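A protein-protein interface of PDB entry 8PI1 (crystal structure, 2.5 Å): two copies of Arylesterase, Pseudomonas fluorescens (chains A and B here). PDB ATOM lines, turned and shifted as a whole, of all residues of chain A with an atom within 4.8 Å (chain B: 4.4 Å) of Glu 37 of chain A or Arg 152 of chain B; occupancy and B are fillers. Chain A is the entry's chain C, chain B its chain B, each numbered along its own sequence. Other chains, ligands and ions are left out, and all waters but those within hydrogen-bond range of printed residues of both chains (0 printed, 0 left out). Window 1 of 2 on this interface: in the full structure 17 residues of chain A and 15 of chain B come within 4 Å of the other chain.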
ATOM      1  N   TRP A  17     -24.772   6.929  11.977  1.00  0.00           N
ATOM      2  CA  TRP A  17     -23.693   6.600  12.899  1.00  0.00           C
ATOM      3  C   TRP A  17     -24.072   5.407  13.773  1.00  0.00           C
ATOM      4  O   TRP A  17     -25.193   5.331  14.274  1.00  0.00           O
ATOM      5  CB  TRP A  17     -23.326   7.803  13.781  1.00  0.00           C
ATOM      6  CG  TRP A  17     -22.584   8.908  13.095  1.00  0.00           C
ATOM      7  CD1 TRP A  17     -22.168   8.947  11.795  1.00  0.00           C
ATOM      8  CD2 TRP A  17     -22.170  10.156  13.685  1.00  0.00           C
ATOM      9  NE1 TRP A  17     -21.527  10.128  11.537  1.00  0.00           N
ATOM     10  CE2 TRP A  17     -21.514  10.892  12.674  1.00  0.00           C
ATOM     11  CE3 TRP A  17     -22.297  10.727  14.958  1.00  0.00           C
ATOM     12  CZ2 TRP A  17     -20.981  12.159  12.904  1.00  0.00           C
ATOM     13  CZ3 TRP A  17     -21.773  11.981  15.185  1.00  0.00           C
ATOM     14  CH2 TRP A  17     -21.121  12.684  14.169  1.00  0.00           C
ATOM     15  N   ALA A  33     -28.243  19.058  10.339  1.00  0.00           N
ATOM     16  CA  ALA A  33     -27.970  17.840  11.088  1.00  0.00           C
ATOM     17  C   ALA A  33     -26.868  18.053  12.123  1.00  0.00           C
ATOM     18  O   ALA A  33     -26.820  17.337  13.119  1.00  0.00           O
ATOM     19  CB  ALA A  33     -27.619  16.716  10.144  1.00  0.00           C
ATOM     20  N   ASP A  34     -25.990  19.036  11.884  1.00  0.00           N
ATOM     21  CA  ASP A  34     -24.826  19.267  12.728  1.00  0.00           C
ATOM     22  C   ASP A  34     -25.221  19.718  14.136  1.00  0.00           C
ATOM     23  O   ASP A  34     -24.398  19.635  15.043  1.00  0.00           O
ATOM     24  CB  ASP A  34     -23.825  20.241  12.096  1.00  0.00           C
ATOM     25  CG  ASP A  34     -23.044  19.689  10.913  1.00  0.00           C
ATOM     26  OD1 ASP A  34     -23.133  18.471  10.653  1.00  0.00           O
ATOM     27  OD2 ASP A  34     -22.358  20.490  10.247  1.00  0.00           O
ATOM     28  N   MET A  35     -26.459  20.197  14.329  1.00  0.00           N
ATOM     29  CA  MET A  35     -26.868  20.659  15.651  1.00  0.00           C
ATOM     30  C   MET A  35     -27.012  19.464  16.594  1.00  0.00           C
ATOM     31  O   MET A  35     -27.122  19.643  17.804  1.00  0.00           O
ATOM     32  CB  MET A  35     -28.191  21.436  15.642  1.00  0.00           C
ATOM     33  CG  MET A  35     -29.404  20.599  15.248  1.00  0.00           C
ATOM     34  SD  MET A  35     -30.981  21.074  16.030  1.00  0.00           S
ATOM     35  CE  MET A  35     -30.544  21.027  17.768  1.00  0.00           C
ATOM     36  N   TRP A  36     -27.010  18.252  16.026  1.00  0.00           N
ATOM     37  CA  TRP A  36     -27.281  17.042  16.785  1.00  0.00           C
ATOM     38  C   TRP A  36     -25.989  16.334  17.186  1.00  0.00           C
ATOM     39  O   TRP A  36     -26.031  15.362  17.942  1.00  0.00           O
ATOM     40  CB  TRP A  36     -28.195  16.109  15.985  1.00  0.00           C
ATOM     41  CG  TRP A  36     -29.605  16.586  15.805  1.00  0.00           C
ATOM     42  CD1 TRP A  36     -30.234  16.849  14.622  1.00  0.00           C
ATOM     43  CD2 TRP A  36     -30.588  16.808  16.836  1.00  0.00           C
ATOM     44  NE1 TRP A  36     -31.530  17.228  14.843  1.00  0.00           N
ATOM     45  CE2 TRP A  36     -31.778  17.213  16.190  1.00  0.00           C
ATOM     46  CE3 TRP A  36     -30.580  16.715  18.234  1.00  0.00           C
ATOM     47  CZ2 TRP A  36     -32.941  17.526  16.896  1.00  0.00           C
ATOM     48  CZ3 TRP A  36     -31.730  17.022  18.931  1.00  0.00           C
ATOM     49  CH2 TRP A  36     -32.893  17.423  18.268  1.00  0.00           C
ATOM     50  N   GLU A  37     -24.847  16.845  16.703  1.00  0.00           N
ATOM     51  CA  GLU A  37     -23.572  16.137  16.734  1.00  0.00           C
ATOM     52  C   GLU A  37     -23.230  15.639  18.140  1.00  0.00           C
ATOM     53  O   GLU A  37     -22.739  14.520  18.291  1.00  0.00           O
ATOM     54  CB  GLU A  37     -22.460  16.978  16.102  1.00  0.00           C
ATOM     55  CG  GLU A  37     -22.228  18.319  16.786  1.00  0.00           C
ATOM     56  CD  GLU A  37     -21.248  19.256  16.096  1.00  0.00           C
ATOM     57  OE1 GLU A  37     -20.722  18.889  15.022  1.00  0.00           O
ATOM     58  OE2 GLU A  37     -21.008  20.357  16.635  1.00  0.00           O
ATOM     59  N   TYR A  38     -23.503  16.462  19.160  1.00  0.00           N
ATOM     60  CA  TYR A  38     -23.152  16.118  20.530  1.00  0.00           C
ATOM     61  C   TYR A  38     -24.031  14.976  21.036  1.00  0.00           C
ATOM     62  O   TYR A  38     -23.525  14.036  21.645  1.00  0.00           O
ATOM     63  CB  TYR A  38     -23.145  17.361  21.426  1.00  0.00           C
ATOM     64  CG  TYR A  38     -22.037  18.334  21.100  1.00  0.00           C
ATOM     65  CD1 TYR A  38     -20.717  18.053  21.424  1.00  0.00           C
ATOM     66  CD2 TYR A  38     -22.302  19.518  20.426  1.00  0.00           C
ATOM     67  CE1 TYR A  38     -19.694  18.932  21.110  1.00  0.00           C
ATOM     68  CE2 TYR A  38     -21.290  20.408  20.103  1.00  0.00           C
ATOM     69  CZ  TYR A  38     -19.982  20.112  20.444  1.00  0.00           C
ATOM     70  OH  TYR A  38     -18.978  20.991  20.123  1.00  0.00           O
ATOM     71  N   GLN A  39     -25.338  15.060  20.759  1.00  0.00           N
ATOM     72  CA  GLN A  39     -26.296  14.037  21.154  1.00  0.00           C
ATOM     73  C   GLN A  39     -25.946  12.718  20.464  1.00  0.00           C
ATOM     74  O   GLN A  39     -25.948  11.661  21.092  1.00  0.00           O
ATOM     75  CB  GLN A  39     -27.721  14.456  20.774  1.00  0.00           C
ATOM     76  CG  GLN A  39     -28.362  15.488  21.696  1.00  0.00           C
ATOM     77  CD  GLN A  39     -27.639  16.813  21.753  1.00  0.00           C
ATOM     78  OE1 GLN A  39     -27.339  17.327  22.829  1.00  0.00           O
ATOM     79  NE2 GLN A  39     -27.361  17.386  20.593  1.00  0.00           N
ATOM     80  N   MET A  40     -25.633  12.808  19.166  1.00  0.00           N
ATOM     81  CA  MET A  40     -25.382  11.649  18.325  1.00  0.00           C
ATOM     82  C   MET A  40     -24.136  10.912  18.810  1.00  0.00           C
ATOM     83  O   MET A  40     -24.170   9.694  18.971  1.00  0.00           O
ATOM     84  CB  MET A  40     -25.208  12.064  16.861  1.00  0.00           C
ATOM     85  CG  MET A  40     -26.528  12.316  16.153  1.00  0.00           C
ATOM     86  SD  MET A  40     -26.298  12.842  14.432  1.00  0.00           S
ATOM     87  CE  MET A  40     -26.129  11.252  13.621  1.00  0.00           C
ATOM     88  N   GLU A  41     -23.049  11.654  19.061  1.00  0.00           N
ATOM     89  CA  GLU A  41     -21.821  11.035  19.540  1.00  0.00           C
ATOM     90  C   GLU A  41     -22.073  10.396  20.904  1.00  0.00           C
ATOM     91  O   GLU A  41     -21.577   9.305  21.174  1.00  0.00           O
ATOM     92  CB  GLU A  41     -20.661  12.032  19.579  1.00  0.00           C
ATOM     93  CG  GLU A  41     -19.315  11.389  19.892  1.00  0.00           C
ATOM     94  CD  GLU A  41     -19.039  11.030  21.344  1.00  0.00           C
ATOM     95  OE1 GLU A  41     -19.664  11.633  22.242  1.00  0.00           O
ATOM     96  OE2 GLU A  41     -18.214  10.122  21.577  1.00  0.00           O
ATOM     97  N   GLN A 179     -20.628  29.152  14.313  1.00  0.00           N
ATOM     98  CA  GLN A 179     -21.031  27.902  13.689  1.00  0.00           C
ATOM     99  C   GLN A 179     -22.517  27.935  13.331  1.00  0.00           C
ATOM    100  O   GLN A 179     -22.925  27.349  12.331  1.00  0.00           O
ATOM    101  CB  GLN A 179     -20.706  26.724  14.609  1.00  0.00           C
ATOM    102  CG  GLN A 179     -21.018  25.371  13.990  1.00  0.00           C
ATOM    103  CD  GLN A 179     -20.792  24.240  14.962  1.00  0.00           C
ATOM    104  OE1 GLN A 179     -20.451  24.449  16.125  1.00  0.00           O
ATOM    105  NE2 GLN A 179     -20.993  23.022  14.486  1.00  0.00           N
ATOM    106  N   GLU B 147     -12.809  18.837  26.078  1.00  0.00           N
ATOM    107  CA  GLU B 147     -13.185  20.183  25.678  1.00  0.00           C
ATOM    108  C   GLU B 147     -13.922  20.137  24.343  1.00  0.00           C
ATOM    109  O   GLU B 147     -14.922  20.833  24.166  1.00  0.00           O
ATOM    110  CB  GLU B 147     -11.965  21.106  25.676  1.00  0.00           C
ATOM    111  CG  GLU B 147     -11.459  21.412  27.077  1.00  0.00           C
ATOM    112  CD  GLU B 147     -10.046  21.966  27.179  1.00  0.00           C
ATOM    113  OE1 GLU B 147      -9.385  22.117  26.128  1.00  0.00           O
ATOM    114  OE2 GLU B 147      -9.606  22.243  28.316  1.00  0.00           O
ATOM    115  N   LEU B 148     -13.426  19.292  23.431  1.00  0.00           N
ATOM    116  CA  LEU B 148     -14.043  19.083  22.130  1.00  0.00           C
ATOM    117  C   LEU B 148     -15.460  18.538  22.298  1.00  0.00           C
ATOM    118  O   LEU B 148     -16.329  18.829  21.481  1.00  0.00           O
ATOM    119  CB  LEU B 148     -13.182  18.113  21.314  1.00  0.00           C
ATOM    120  CG  LEU B 148     -11.904  18.688  20.701  1.00  0.00           C
ATOM    121  CD1 LEU B 148     -10.998  17.569  20.211  1.00  0.00           C
ATOM    122  CD2 LEU B 148     -12.227  19.633  19.550  1.00  0.00           C
ATOM    123  N   LYS B 150     -17.441  19.292  24.635  1.00  0.00           N
ATOM    124  CA  LYS B 150     -18.270  20.320  25.247  1.00  0.00           C
ATOM    125  C   LYS B 150     -18.586  21.405  24.223  1.00  0.00           C
ATOM    126  O   LYS B 150     -19.746  21.772  24.046  1.00  0.00           O
ATOM    127  CB  LYS B 150     -17.608  20.882  26.510  1.00  0.00           C
ATOM    128  CG  LYS B 150     -17.607  19.928  27.695  1.00  0.00           C
ATOM    129  CD  LYS B 150     -16.928  20.454  28.939  1.00  0.00           C
ATOM    130  CE  LYS B 150     -17.014  19.456  30.075  1.00  0.00           C
ATOM    131  NZ  LYS B 150     -16.220  19.881  31.251  1.00  0.00           N
ATOM    132  N   ASP B 151     -17.539  21.892  23.543  1.00  0.00           N
ATOM    133  CA  ASP B 151     -17.654  22.982  22.587  1.00  0.00           C
ATOM    134  C   ASP B 151     -16.455  22.931  21.645  1.00  0.00           C
ATOM    135  O   ASP B 151     -15.430  23.552  21.910  1.00  0.00           O
ATOM    136  CB  ASP B 151     -17.766  24.325  23.320  1.00  0.00           C
ATOM    137  CG  ASP B 151     -17.892  25.552  22.428  1.00  0.00           C
ATOM    138  OD1 ASP B 151     -17.744  25.420  21.190  1.00  0.00           O
ATOM    139  OD2 ASP B 151     -18.144  26.640  22.986  1.00  0.00           O
ATOM    140  N   ARG B 152     -16.590  22.193  20.538  1.00  0.00           N
ATOM    141  CA  ARG B 152     -15.473  22.048  19.620  1.00  0.00           C
ATOM    142  C   ARG B 152     -15.240  23.359  18.871  1.00  0.00           C
ATOM    143  O   ARG B 152     -14.108  23.673  18.514  1.00  0.00           O
ATOM    144  CB  ARG B 152     -15.650  20.864  18.661  1.00  0.00           C
ATOM    145  CG  ARG B 152     -16.656  21.088  17.541  1.00  0.00           C
ATOM    146  CD  ARG B 152     -16.543  20.006  16.486  1.00  0.00           C
ATOM    147  NE  ARG B 152     -17.648  20.063  15.537  1.00  0.00           N
ATOM    148  CZ  ARG B 152     -17.511  20.173  14.221  1.00  0.00           C
ATOM    149  NH1 ARG B 152     -16.306  20.244  13.678  1.00  0.00           N
ATOM    150  NH2 ARG B 152     -18.586  20.213  13.452  1.00  0.00           N
ATOM    151  N   ALA B 153     -16.322  24.116  18.652  1.00  0.00           N
ATOM    152  CA  ALA B 153     -16.273  25.338  17.867  1.00  0.00           C
ATOM    153  C   ALA B 153     -15.323  26.347  18.511  1.00  0.00           C
ATOM    154  O   ALA B 153     -14.507  26.950  17.819  1.00  0.00           O
ATOM    155  CB  ALA B 153     -17.665  25.897  17.705  1.00  0.00           C
ATOM    156  N   GLN B 154     -15.420  26.505  19.837  1.00  0.00           N
ATOM    157  CA  GLN B 154     -14.566  27.434  20.561  1.00  0.00           C
ATOM    158  C   GLN B 154     -13.145  26.877  20.659  1.00  0.00           C
ATOM    159  O   GLN B 154     -12.180  27.632  20.559  1.00  0.00           O
ATOM    160  CB  GLN B 154     -15.175  27.784  21.922  1.00  0.00           C
ATOM    161  CG  GLN B 154     -14.559  29.010  22.590  1.00  0.00           C
ATOM    162  CD  GLN B 154     -14.409  30.211  21.683  1.00  0.00           C
ATOM    163  OE1 GLN B 154     -15.334  30.614  20.979  1.00  0.00           O
ATOM    164  NE2 GLN B 154     -13.223  30.797  21.689  1.00  0.00           N
ATOM    165  N   PHE B 155     -13.019  25.555  20.829  1.00  0.00           N
ATOM    166  CA  PHE B 155     -11.712  24.922  20.944  1.00  0.00           C
ATOM    167  C   PHE B 155     -10.866  25.225  19.708  1.00  0.00           C
ATOM    168  O   PHE B 155      -9.699  25.591  19.841  1.00  0.00           O
ATOM    169  CB  PHE B 155     -11.828  23.416  21.206  1.00  0.00           C
ATOM    170  CG  PHE B 155     -10.510  22.682  21.278  1.00  0.00           C
ATOM    171  CD1 PHE B 155      -9.795  22.375  20.126  1.00  0.00           C
ATOM    172  CD2 PHE B 155      -9.970  22.316  22.504  1.00  0.00           C
ATOM    173  CE1 PHE B 155      -8.575  21.716  20.196  1.00  0.00           C
ATOM    174  CE2 PHE B 155      -8.754  21.650  22.574  1.00  0.00           C
ATOM    175  CZ  PHE B 155      -8.057  21.354  21.422  1.00  0.00           C
ATOM    176  N   ILE B 156     -11.469  25.064  18.522  1.00  0.00           N
ATOM    177  CA  ILE B 156     -10.803  25.313  17.251  1.00  0.00           C
ATOM    178  C   ILE B 156     -10.355  26.771  17.202  1.00  0.00           C
ATOM    179  O   ILE B 156      -9.229  27.061  16.802  1.00  0.00           O
ATOM    180  CB  ILE B 156     -11.718  24.978  16.056  1.00  0.00           C
ATOM    181  CG1 ILE B 156     -12.242  23.541  16.110  1.00  0.00           C
ATOM    182  CG2 ILE B 156     -10.999  25.259  14.745  1.00  0.00           C
ATOM    183  CD1 ILE B 156     -13.474  23.299  15.259  1.00  0.00           C
ATOM    184  N   ALA B 184     -12.684  23.904   9.556  1.00  0.00           N
ATOM    185  CA  ALA B 184     -12.673  22.964  10.665  1.00  0.00           C
ATOM    186  C   ALA B 184     -14.096  22.601  11.080  1.00  0.00           C
ATOM    187  O   ALA B 184     -14.335  21.500  11.577  1.00  0.00           O
ATOM    188  CB  ALA B 184     -11.890  23.534  11.817  1.00  0.00           C
ATOM    189  N   LEU B 185     -15.032  23.530  10.849  1.00  0.00           N
ATOM    190  CA  LEU B 185     -16.414  23.352  11.262  1.00  0.00           C
ATOM    191  C   LEU B 185     -17.161  22.436  10.294  1.00  0.00           C
ATOM    192  O   LEU B 185     -18.239  21.944  10.623  1.00  0.00           O
ATOM    193  CB  LEU B 185     -17.083  24.725  11.390  1.00  0.00           C
ATOM    194  CG  LEU B 185     -16.732  25.504  12.659  1.00  0.00           C
ATOM    195  CD1 LEU B 185     -17.463  26.836  12.708  1.00  0.00           C
ATOM    196  CD2 LEU B 185     -17.050  24.689  13.904  1.00  0.00           C
ATOM    197  N   ALA B 187     -16.008  19.609   9.413  1.00  0.00           N
ATOM    198  CA  ALA B 187     -15.605  18.277   9.835  1.00  0.00           C
ATOM    199  C   ALA B 187     -16.596  17.688  10.839  1.00  0.00           C
ATOM    200  O   ALA B 187     -17.360  18.409  11.476  1.00  0.00           O
ATOM    201  CB  ALA B 187     -14.215  18.343  10.417  1.00  0.00           C
ATOM    202  N   LEU B 189     -17.696  15.825  14.311  1.00  0.00           N
ATOM    203  CA  LEU B 189     -17.305  15.818  15.711  1.00  0.00           C
ATOM    204  C   LEU B 189     -16.625  14.492  16.049  1.00  0.00           C
ATOM    205  O   LEU B 189     -15.657  14.463  16.811  1.00  0.00           O
ATOM    206  CB  LEU B 189     -18.544  16.039  16.585  1.00  0.00           C
ATOM    207  CG  LEU B 189     -18.320  15.857  18.086  1.00  0.00           C
ATOM    208  CD1 LEU B 189     -17.460  16.980  18.648  1.00  0.00           C
ATOM    209  CD2 LEU B 189     -19.646  15.763  18.829  1.00  0.00           C
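The side-chain hydroxyl of Tyr 38 of chain A is in hydrogen-bond range of the backbone NH of Arg 152 of chain B (2.7 Å).
The side-chain carboxylate (OE1) of Glu 37 of chain A is in salt-bridge range of the guanidinium group (NH2) of Arg 152 of chain B (3.0 Å).
The backbone carbonyl oxygen of Ala 184 of chain B lies within hydrogen-bond range of the guanidinium group of Arg 152 of chain B (3.1 Å).
The guanidinium group (NH2) of Arg 152 of chain B sits at hydrogen-bond distance from the backbone carbonyl oxygen (O) of Leu 185 of chain B (3.3 Å).
The guanidinium group (NH2) of Arg 152 of chain B sits at hydrogen-bond distance from the backbone carbonyl oxygen (O) of Ala 187 of chain B, 2.9 Å away.
OD1 of Asp 151 of chain B lies within hydrogen-bond range of N of Gln 154 of chain B, 2.9 Å away.
The side-chain carboxylate (OE2) of Glu 37 of chain A lies within hydrogen-bond range of the side-chain amide nitrogen (NE2) of Gln 179 of chain A (3.4 Å).
N of Ala 153 of chain B lies within hydrogen-bond range of OD1 of Asp 151 of chain B (3.2 Å).
Among the printed residues, merely in contact across the chains: Glu 37 of chain A with Leu 189 of chain B (3.4 Å), Tyr 38 of chain A with Leu 148 of chain B (3.4 Å), Tyr 38 of chain A with Asp 151 of chain B (3.4 Å), Gln 179 of chain A with Ala 153 of chain B (3.5 Å), Tyr 38 of chain A with Leu 189 of chain B (3.6 Å), Gln 179 of chain A with Leu 185 of chain B (3.8 Å), Gln 179 of chain A with Arg 152 of chain B (3.8 Å), Glu 41 of chain A with Leu 189 of chain B (3.9 Å) and Tyr 38 of chain A with Lys 150 of chain B (3.97 Å).
Glu 37 of chain A touches just these residues of chain B: Arg 152 (3.0 Å) and Leu 189 (3.4 Å).
Of chain A, only Glu 37, Tyr 38 and Gln 179 come within 4 Å of Arg 152 of chain B.
Of the printed residues of chain B, Tyr 38 of chain A touches Leu 148 (3.4 Å), Lys 150 (3.97 Å), Asp 151 (3.4 Å), Arg 152 (2.7 Å) and Leu 189 (3.6 Å).
Of the printed residues of chain B, Glu 41 of chain A touches Leu 189 (3.9 Å).
Printed residues of chain A within 4 Å of Lys 150 of chain B: Tyr 38 (3.97 Å).
Met 35 of chain A touches none of the printed residues of chain B.
The nearest printed residue of chain A that does not touch Arg 152 of chain B is Asp 34 of chain A (5.0 Å).
Of the 13 printed residues of chain B, 7 touch a printed residue of chain A.
Printed residues of chain B that touch a printed residue of chain A: Leu 148, Lys 150, Asp 151, Arg 152, Ala 153, Leu 185 and Leu 189.
Hydrophobic or aromatic side chains of chain B within 4 Å of the printed part of chain A: Ala 153, Leu 185 and Leu 189.
Hydrophobic or aromatic side chains of chain A within 4 Å of the printed part of chain B: Tyr 38.
Among the printed residues, 11 pairs touch across the chains.
Among the printed residues, Asp or Glu carboxylates within 4 Å of a Lys or Arg side-chain nitrogen of the other chain: Glu 37 of chain A with Arg 152 of chain B (3.0 Å).
No position is printed for both chains.
Of the 11 pairs that touch across the chains among the printed residues, none has its exchanged pair printed and touching as well.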
